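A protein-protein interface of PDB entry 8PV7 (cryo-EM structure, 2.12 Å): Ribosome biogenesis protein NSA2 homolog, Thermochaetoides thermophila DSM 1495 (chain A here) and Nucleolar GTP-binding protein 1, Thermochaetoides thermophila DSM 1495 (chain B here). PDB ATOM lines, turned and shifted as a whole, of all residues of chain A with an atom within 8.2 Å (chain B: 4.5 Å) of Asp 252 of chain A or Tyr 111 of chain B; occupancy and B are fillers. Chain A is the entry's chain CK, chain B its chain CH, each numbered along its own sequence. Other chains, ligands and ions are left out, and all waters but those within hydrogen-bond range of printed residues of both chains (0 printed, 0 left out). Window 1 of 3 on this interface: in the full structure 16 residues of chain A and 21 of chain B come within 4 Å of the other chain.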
ATOM      1  N   PRO A 154      -8.856  16.519  10.546  1.00  0.00           N
ATOM      2  CA  PRO A 154      -7.482  16.018  10.688  1.00  0.00           C
ATOM      3  C   PRO A 154      -6.501  16.699   9.743  1.00  0.00           C
ATOM      4  O   PRO A 154      -6.812  16.969   8.584  1.00  0.00           O
ATOM      5  CB  PRO A 154      -7.621  14.531  10.357  1.00  0.00           C
ATOM      6  CG  PRO A 154      -9.006  14.210  10.699  1.00  0.00           C
ATOM      7  CD  PRO A 154      -9.809  15.411  10.353  1.00  0.00           C
ATOM      8  N   GLY A 176      -4.158  16.339  18.886  1.00  0.00           N
ATOM      9  CA  GLY A 176      -4.965  15.139  18.839  1.00  0.00           C
ATOM     10  C   GLY A 176      -5.575  14.850  17.492  1.00  0.00           C
ATOM     11  O   GLY A 176      -6.075  13.741  17.286  1.00  0.00           O
ATOM     12  N   TYR A 179      -2.129  13.663  12.108  1.00  0.00           N
ATOM     13  CA  TYR A 179      -1.901  12.307  11.636  1.00  0.00           C
ATOM     14  C   TYR A 179      -0.578  12.227  10.895  1.00  0.00           C
ATOM     15  O   TYR A 179      -0.116  13.204  10.301  1.00  0.00           O
ATOM     16  CB  TYR A 179      -3.018  11.831  10.706  1.00  0.00           C
ATOM     17  CG  TYR A 179      -4.270  11.398  11.412  1.00  0.00           C
ATOM     18  CD1 TYR A 179      -5.199  12.327  11.838  1.00  0.00           C
ATOM     19  CD2 TYR A 179      -4.516  10.059  11.673  1.00  0.00           C
ATOM     20  CE1 TYR A 179      -6.340  11.941  12.490  1.00  0.00           C
ATOM     21  CE2 TYR A 179      -5.659   9.662  12.328  1.00  0.00           C
ATOM     22  CZ  TYR A 179      -6.566  10.610  12.736  1.00  0.00           C
ATOM     23  OH  TYR A 179      -7.712  10.236  13.387  1.00  0.00           O
ATOM     24  N   ILE A 245      -7.258  10.358  -0.838  1.00  0.00           N
ATOM     25  CA  ILE A 245      -8.001   9.942   0.345  1.00  0.00           C
ATOM     26  C   ILE A 245      -9.429   9.594  -0.049  1.00  0.00           C
ATOM     27  O   ILE A 245     -10.133  10.397  -0.672  1.00  0.00           O
ATOM     28  CB  ILE A 245      -7.962  11.042   1.415  1.00  0.00           C
ATOM     29  CG1 ILE A 245      -6.531  11.235   1.929  1.00  0.00           C
ATOM     30  CG2 ILE A 245      -8.928  10.742   2.548  1.00  0.00           C
ATOM     31  CD1 ILE A 245      -6.372  12.356   2.928  1.00  0.00           C
ATOM     32  N   THR A 246      -9.868   8.397   0.323  1.00  0.00           N
ATOM     33  CA  THR A 246     -11.157   7.877  -0.106  1.00  0.00           C
ATOM     34  C   THR A 246     -12.205   7.833   0.992  1.00  0.00           C
ATOM     35  O   THR A 246     -13.321   7.377   0.736  1.00  0.00           O
ATOM     36  CB  THR A 246     -10.985   6.475  -0.692  1.00  0.00           C
ATOM     37  OG1 THR A 246     -10.288   5.644   0.241  1.00  0.00           O
ATOM     38  CG2 THR A 246     -10.206   6.548  -1.976  1.00  0.00           C
ATOM     39  N   ASN A 247     -11.896   8.308   2.191  1.00  0.00           N
ATOM     40  CA  ASN A 247     -12.830   8.239   3.303  1.00  0.00           C
ATOM     41  C   ASN A 247     -12.976   9.618   3.928  1.00  0.00           C
ATOM     42  O   ASN A 247     -12.385  10.595   3.470  1.00  0.00           O
ATOM     43  CB  ASN A 247     -12.370   7.213   4.345  1.00  0.00           C
ATOM     44  CG  ASN A 247     -11.187   7.691   5.165  1.00  0.00           C
ATOM     45  OD1 ASN A 247     -10.229   8.243   4.635  1.00  0.00           O
ATOM     46  ND2 ASN A 247     -11.259   7.493   6.469  1.00  0.00           N
ATOM     47  N   ASN A 248     -13.767   9.689   4.994  1.00  0.00           N
ATOM     48  CA  ASN A 248     -13.867  10.901   5.797  1.00  0.00           C
ATOM     49  C   ASN A 248     -13.135  10.676   7.114  1.00  0.00           C
ATOM     50  O   ASN A 248     -13.691  10.060   8.038  1.00  0.00           O
ATOM     51  CB  ASN A 248     -15.330  11.271   6.044  1.00  0.00           C
ATOM     52  CG  ASN A 248     -16.030  11.742   4.786  1.00  0.00           C
ATOM     53  OD1 ASN A 248     -15.603  12.700   4.151  1.00  0.00           O
ATOM     54  ND2 ASN A 248     -17.110  11.070   4.422  1.00  0.00           N
ATOM     55  N   PRO A 249     -11.882  11.125   7.234  1.00  0.00           N
ATOM     56  CA  PRO A 249     -11.114  10.864   8.463  1.00  0.00           C
ATOM     57  C   PRO A 249     -11.691  11.496   9.714  1.00  0.00           C
ATOM     58  O   PRO A 249     -11.516  10.933  10.801  1.00  0.00           O
ATOM     59  CB  PRO A 249      -9.731  11.436   8.129  1.00  0.00           C
ATOM     60  CG  PRO A 249      -9.661  11.414   6.658  1.00  0.00           C
ATOM     61  CD  PRO A 249     -11.041  11.728   6.190  1.00  0.00           C
ATOM     62  N   GLU A 250     -12.377  12.638   9.599  1.00  0.00           N
ATOM     63  CA  GLU A 250     -12.965  13.275  10.773  1.00  0.00           C
ATOM     64  C   GLU A 250     -14.099  12.443  11.356  1.00  0.00           C
ATOM     65  O   GLU A 250     -14.420  12.575  12.540  1.00  0.00           O
ATOM     66  CB  GLU A 250     -13.465  14.680  10.423  1.00  0.00           C
ATOM     67  CG  GLU A 250     -14.735  14.733   9.583  1.00  0.00           C
ATOM     68  CD  GLU A 250     -14.483  14.592   8.093  1.00  0.00           C
ATOM     69  OE1 GLU A 250     -13.314  14.438   7.684  1.00  0.00           O
ATOM     70  OE2 GLU A 250     -15.462  14.645   7.328  1.00  0.00           O
ATOM     71  N   ASN A 251     -14.709  11.578  10.550  1.00  0.00           N
ATOM     72  CA  ASN A 251     -15.740  10.675  11.028  1.00  0.00           C
ATOM     73  C   ASN A 251     -15.212   9.291  11.359  1.00  0.00           C
ATOM     74  O   ASN A 251     -15.786   8.620  12.223  1.00  0.00           O
ATOM     75  CB  ASN A 251     -16.861  10.541   9.991  1.00  0.00           C
ATOM     76  CG  ASN A 251     -17.645  11.814   9.817  1.00  0.00           C
ATOM     77  OD1 ASN A 251     -17.484  12.762  10.578  1.00  0.00           O
ATOM     78  ND2 ASN A 251     -18.508  11.842   8.814  1.00  0.00           N
ATOM     79  N   ASP A 252     -14.138   8.851  10.710  1.00  0.00           N
ATOM     80  CA  ASP A 252     -13.671   7.485  10.889  1.00  0.00           C
ATOM     81  C   ASP A 252     -12.575   7.334  11.932  1.00  0.00           C
ATOM     82  O   ASP A 252     -12.459   6.261  12.528  1.00  0.00           O
ATOM     83  CB  ASP A 252     -13.166   6.922   9.559  1.00  0.00           C
ATOM     84  CG  ASP A 252     -14.268   6.785   8.534  1.00  0.00           C
ATOM     85  OD1 ASP A 252     -13.956   6.692   7.332  1.00  0.00           O
ATOM     86  OD2 ASP A 252     -15.451   6.775   8.930  1.00  0.00           O
ATOM     87  N   GLY A 253     -11.771   8.363  12.172  1.00  0.00           N
ATOM     88  CA  GLY A 253     -10.625   8.184  13.030  1.00  0.00           C
ATOM     89  C   GLY A 253      -9.434   7.526  12.375  1.00  0.00           C
ATOM     90  O   GLY A 253      -8.528   7.078  13.083  1.00  0.00           O
ATOM     91  N   CYS A 254      -9.411   7.442  11.049  1.00  0.00           N
ATOM     92  CA  CYS A 254      -8.278   6.899  10.319  1.00  0.00           C
ATOM     93  C   CYS A 254      -8.248   7.542   8.942  1.00  0.00           C
ATOM     94  O   CYS A 254      -9.234   8.126   8.492  1.00  0.00           O
ATOM     95  CB  CYS A 254      -8.353   5.373  10.201  1.00  0.00           C
ATOM     96  SG  CYS A 254      -9.811   4.765   9.331  1.00  0.00           S
ATOM     97  N   VAL A 255      -7.107   7.434   8.274  1.00  0.00           N
ATOM     98  CA  VAL A 255      -6.952   7.922   6.910  1.00  0.00           C
ATOM     99  C   VAL A 255      -6.859   6.717   5.986  1.00  0.00           C
ATOM    100  O   VAL A 255      -5.972   5.873   6.142  1.00  0.00           O
ATOM    101  CB  VAL A 255      -5.722   8.828   6.760  1.00  0.00           C
ATOM    102  CG1 VAL A 255      -5.654   9.379   5.350  1.00  0.00           C
ATOM    103  CG2 VAL A 255      -5.759   9.957   7.774  1.00  0.00           C
ATOM    104  N   ASN A 256      -7.780   6.638   5.032  1.00  0.00           N
ATOM    105  CA  ASN A 256      -7.783   5.612   4.000  1.00  0.00           C
ATOM    106  C   ASN A 256      -7.501   6.257   2.653  1.00  0.00           C
ATOM    107  O   ASN A 256      -8.100   7.278   2.309  1.00  0.00           O
ATOM    108  CB  ASN A 256      -9.127   4.887   3.941  1.00  0.00           C
ATOM    109  CG  ASN A 256      -9.403   4.060   5.170  1.00  0.00           C
ATOM    110  OD1 ASN A 256      -8.488   3.603   5.845  1.00  0.00           O
ATOM    111  ND2 ASN A 256     -10.676   3.856   5.467  1.00  0.00           N
ATOM    112  N   ILE B 107      -7.326   2.133  21.527  1.00  0.00           N
ATOM    113  CA  ILE B 107      -8.416   2.585  20.664  1.00  0.00           C
ATOM    114  C   ILE B 107      -9.343   3.522  21.427  1.00  0.00           C
ATOM    115  O   ILE B 107      -9.769   4.568  20.913  1.00  0.00           O
ATOM    116  CB  ILE B 107      -9.173   1.370  20.099  1.00  0.00           C
ATOM    117  CG1 ILE B 107      -8.413   0.771  18.922  1.00  0.00           C
ATOM    118  CG2 ILE B 107     -10.600   1.723  19.699  1.00  0.00           C
ATOM    119  CD1 ILE B 107      -9.047  -0.465  18.391  1.00  0.00           C
ATOM    120  N   SER B 108      -9.649   3.165  22.676  1.00  0.00           N
ATOM    121  CA  SER B 108     -10.506   4.000  23.509  1.00  0.00           C
ATOM    122  C   SER B 108      -9.893   5.373  23.753  1.00  0.00           C
ATOM    123  O   SER B 108     -10.587   6.391  23.662  1.00  0.00           O
ATOM    124  CB  SER B 108     -10.769   3.298  24.830  1.00  0.00           C
ATOM    125  OG  SER B 108     -11.591   4.070  25.680  1.00  0.00           O
ATOM    126  N   ARG B 109      -8.591   5.420  24.058  1.00  0.00           N
ATOM    127  CA  ARG B 109      -7.943   6.709  24.298  1.00  0.00           C
ATOM    128  C   ARG B 109      -7.949   7.581  23.048  1.00  0.00           C
ATOM    129  O   ARG B 109      -8.238   8.785  23.126  1.00  0.00           O
ATOM    130  CB  ARG B 109      -6.512   6.509  24.790  1.00  0.00           C
ATOM    131  CG  ARG B 109      -6.403   5.957  26.190  1.00  0.00           C
ATOM    132  CD  ARG B 109      -4.994   6.130  26.720  1.00  0.00           C
ATOM    133  NE  ARG B 109      -4.002   5.671  25.757  1.00  0.00           N
ATOM    134  CZ  ARG B 109      -3.482   4.453  25.739  1.00  0.00           C
ATOM    135  NH1 ARG B 109      -3.822   3.544  26.636  1.00  0.00           N
ATOM    136  NH2 ARG B 109      -2.602   4.139  24.794  1.00  0.00           N
ATOM    137  N   ASP B 110      -7.666   6.982  21.886  1.00  0.00           N
ATOM    138  CA  ASP B 110      -7.649   7.735  20.633  1.00  0.00           C
ATOM    139  C   ASP B 110      -9.020   8.315  20.301  1.00  0.00           C
ATOM    140  O   ASP B 110      -9.143   9.492  19.934  1.00  0.00           O
ATOM    141  CB  ASP B 110      -7.164   6.836  19.498  1.00  0.00           C
ATOM    142  CG  ASP B 110      -5.698   6.497  19.613  1.00  0.00           C
ATOM    143  OD1 ASP B 110      -4.976   7.221  20.327  1.00  0.00           O
ATOM    144  OD2 ASP B 110      -5.268   5.496  19.006  1.00  0.00           O
ATOM    145  N   TYR B 111     -10.072   7.512  20.448  1.00  0.00           N
ATOM    146  CA  TYR B 111     -11.386   8.007  20.061  1.00  0.00           C
ATOM    147  C   TYR B 111     -11.974   8.959  21.095  1.00  0.00           C
ATOM    148  O   TYR B 111     -12.758   9.837  20.730  1.00  0.00           O
ATOM    149  CB  TYR B 111     -12.319   6.835  19.778  1.00  0.00           C
ATOM    150  CG  TYR B 111     -12.103   6.282  18.388  1.00  0.00           C
ATOM    151  CD1 TYR B 111     -12.788   6.793  17.296  1.00  0.00           C
ATOM    152  CD2 TYR B 111     -11.177   5.279  18.163  1.00  0.00           C
ATOM    153  CE1 TYR B 111     -12.574   6.299  16.030  1.00  0.00           C
ATOM    154  CE2 TYR B 111     -10.956   4.781  16.906  1.00  0.00           C
ATOM    155  CZ  TYR B 111     -11.655   5.294  15.840  1.00  0.00           C
ATOM    156  OH  TYR B 111     -11.431   4.792  14.584  1.00  0.00           O
ATOM    157  N   VAL B 112     -11.596   8.835  22.369  1.00  0.00           N
ATOM    158  CA  VAL B 112     -11.982   9.849  23.349  1.00  0.00           C
ATOM    159  C   VAL B 112     -11.310  11.181  23.027  1.00  0.00           C
ATOM    160  O   VAL B 112     -11.945  12.251  23.081  1.00  0.00           O
ATOM    161  CB  VAL B 112     -11.651   9.357  24.771  1.00  0.00           C
ATOM    162  CG1 VAL B 112     -11.577  10.509  25.753  1.00  0.00           C
ATOM    163  CG2 VAL B 112     -12.683   8.348  25.219  1.00  0.00           C
ATOM    164  N   ARG B 113     -10.034  11.133  22.633  1.00  0.00           N
ATOM    165  CA  ARG B 113      -9.341  12.347  22.220  1.00  0.00           C
ATOM    166  C   ARG B 113      -9.994  12.986  20.991  1.00  0.00           C
ATOM    167  O   ARG B 113     -10.103  14.213  20.916  1.00  0.00           O
ATOM    168  CB  ARG B 113      -7.868  12.038  21.961  1.00  0.00           C
ATOM    169  CG  ARG B 113      -6.988  13.264  21.903  1.00  0.00           C
ATOM    170  CD  ARG B 113      -5.526  12.920  21.713  1.00  0.00           C
ATOM    171  NE  ARG B 113      -5.019  12.019  22.739  1.00  0.00           N
ATOM    172  CZ  ARG B 113      -4.653  10.766  22.516  1.00  0.00           C
ATOM    173  NH1 ARG B 113      -4.717  10.232  21.309  1.00  0.00           N
ATOM    174  NH2 ARG B 113      -4.208  10.031  23.529  1.00  0.00           N
ATOM    175  N   LEU B 114     -10.454  12.175  20.030  1.00  0.00           N
ATOM    176  CA  LEU B 114     -11.136  12.738  18.858  1.00  0.00           C
ATOM    177  C   LEU B 114     -12.511  13.301  19.216  1.00  0.00           C
ATOM    178  O   LEU B 114     -12.936  14.339  18.678  1.00  0.00           O
ATOM    179  CB  LEU B 114     -11.264  11.683  17.760  1.00  0.00           C
ATOM    180  CG  LEU B 114      -9.960  11.160  17.166  1.00  0.00           C
ATOM    181  CD1 LEU B 114     -10.234  10.077  16.149  1.00  0.00           C
ATOM    182  CD2 LEU B 114      -9.138  12.277  16.563  1.00  0.00           C
ATOM    183  N   LEU B 115     -13.221  12.632  20.126  1.00  0.00           N
ATOM    184  CA  LEU B 115     -14.525  13.116  20.556  1.00  0.00           C
ATOM    185  C   LEU B 115     -14.421  14.433  21.305  1.00  0.00           C
ATOM    186  O   LEU B 115     -15.403  15.172  21.382  1.00  0.00           O
ATOM    187  CB  LEU B 115     -15.213  12.069  21.424  1.00  0.00           C
ATOM    188  CG  LEU B 115     -15.967  11.000  20.641  1.00  0.00           C
ATOM    189  CD1 LEU B 115     -16.500   9.935  21.567  1.00  0.00           C
ATOM    190  CD2 LEU B 115     -17.088  11.638  19.859  1.00  0.00           C
ATOM    191  N   LEU B 127     -17.878   8.547  15.176  1.00  0.00           N
ATOM    192  CA  LEU B 127     -16.659   8.207  15.909  1.00  0.00           C
ATOM    193  C   LEU B 127     -16.921   7.149  16.977  1.00  0.00           C
ATOM    194  O   LEU B 127     -16.094   6.248  17.181  1.00  0.00           O
ATOM    195  CB  LEU B 127     -16.052   9.464  16.527  1.00  0.00           C
ATOM    196  CG  LEU B 127     -15.440  10.467  15.548  1.00  0.00           C
ATOM    197  CD1 LEU B 127     -15.125  11.769  16.253  1.00  0.00           C
ATOM    198  CD2 LEU B 127     -14.204   9.893  14.882  1.00  0.00           C
ATOM    199  N   ALA B 130     -17.270   3.887  15.153  1.00  0.00           N
ATOM    200  CA  ALA B 130     -15.951   3.465  14.699  1.00  0.00           C
ATOM    201  C   ALA B 130     -15.159   2.809  15.823  1.00  0.00           C
ATOM    202  O   ALA B 130     -14.557   1.744  15.629  1.00  0.00           O
ATOM    203  CB  ALA B 130     -15.187   4.658  14.133  1.00  0.00           C
ATOM    204  N   ALA B 131     -15.175   3.419  17.012  1.00  0.00           N
ATOM    205  CA  ALA B 131     -14.463   2.848  18.153  1.00  0.00           C
ATOM    206  C   ALA B 131     -15.029   1.485  18.535  1.00  0.00           C
ATOM    207  O   ALA B 131     -14.276   0.520  18.726  1.00  0.00           O
ATOM    208  CB  ALA B 131     -14.528   3.805  19.341  1.00  0.00           C
ATOM    209  N   ARG B 134     -14.128  -1.195  15.860  1.00  0.00           N
ATOM    210  CA  ARG B 134     -12.734  -1.629  15.923  1.00  0.00           C
ATOM    211  C   ARG B 134     -12.480  -2.537  17.125  1.00  0.00           C
ATOM    212  O   ARG B 134     -11.743  -3.530  17.012  1.00  0.00           O
ATOM    213  CB  ARG B 134     -11.818  -0.410  15.928  1.00  0.00           C
ATOM    214  CG  ARG B 134     -11.820   0.288  14.586  1.00  0.00           C
ATOM    215  CD  ARG B 134     -10.923   1.493  14.520  1.00  0.00           C
ATOM    216  NE  ARG B 134      -9.519   1.153  14.680  1.00  0.00           N
ATOM    217  CZ  ARG B 134      -8.524   2.009  14.503  1.00  0.00           C
ATOM    218  NH1 ARG B 134      -8.744   3.253  14.115  1.00  0.00           N
ATOM    219  NH2 ARG B 134      -7.279   1.612  14.736  1.00  0.00           N
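O of Asp 252 of chain A lies within hydrogen-bond range of OH of Tyr 111 of chain B, 2.7 Å away.
O of Gly 253 of chain A lies within hydrogen-bond range of OH of Tyr 179 of chain A, at 3.3 Å. ND2 of Asn 247 of chain A is in hydrogen-bond range of OD1 of Asp 252 of chain A (2.9 Å). OD1 of Asp 110 of chain B lies within salt-bridge range of NH1 of Arg 113 of chain B (3.2 Å). The side-chain hydroxyl of Tyr 111 of chain B sits at hydrogen-bond distance from the guanidinium group of Arg 134 of chain B, at 3.1 Å.
CD of Arg 113 of chain B touches CA of Gly 176 of chain A, 3.7 Å away. O of Gly 176 of chain A touches CD2 of Leu 114 of chain B (3.5 Å). Tyr 179 of chain A touches Leu 114 of chain B (OH to CD1, 3.7 Å). Leu 127 of chain B touches Glu 250 of chain A. Leu 127 of chain B touches Asn 251 of chain A (CD2 to O, 3.3 Å). Ala 130 of chain B touches Asp 252 of chain A. Gly 253 of chain A touches Tyr 111 of chain B (CA to OH, 3.8 Å). CA of Gly 253 of chain A touches CD1 of Leu 114 of chain B, at 3.7 Å. Leu 127 of chain B touches Gly 253 of chain A. NH1 of Arg 134 of chain B touches O of Gly 253 of chain A, 3.97 Å away.
Asp 252 of chain A touches just these residues of chain B: Tyr 111 and Ala 130. Tyr 111 of chain B touches just these residues of chain A: Asp 252 (2.7 Å) and Gly 253 (3.8 Å). Printed residues of chain B within 4 Å of Glu 250 of chain A: Leu 127 (3.6 Å). Printed residues of chain B within 4 Å of Gly 176 of chain A: Arg 113 (3.7 Å) and Leu 114 (3.5 Å). Printed residues of chain A within 4 Å of Leu 114 of chain B: Gly 176, Tyr 179 and Gly 253. Pro 249 of chain A touches none of the printed residues of chain B. The nearest residue of chain A that does not touch Tyr 111 of chain B is Cys 254 of chain A (4.9 Å).
Hydrophobic or aromatic side chains of chain A within 4 Å of the printed part of chain B: Tyr 179. Of the 13 printed residues of chain B, 6 touch a printed residue of chain A.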
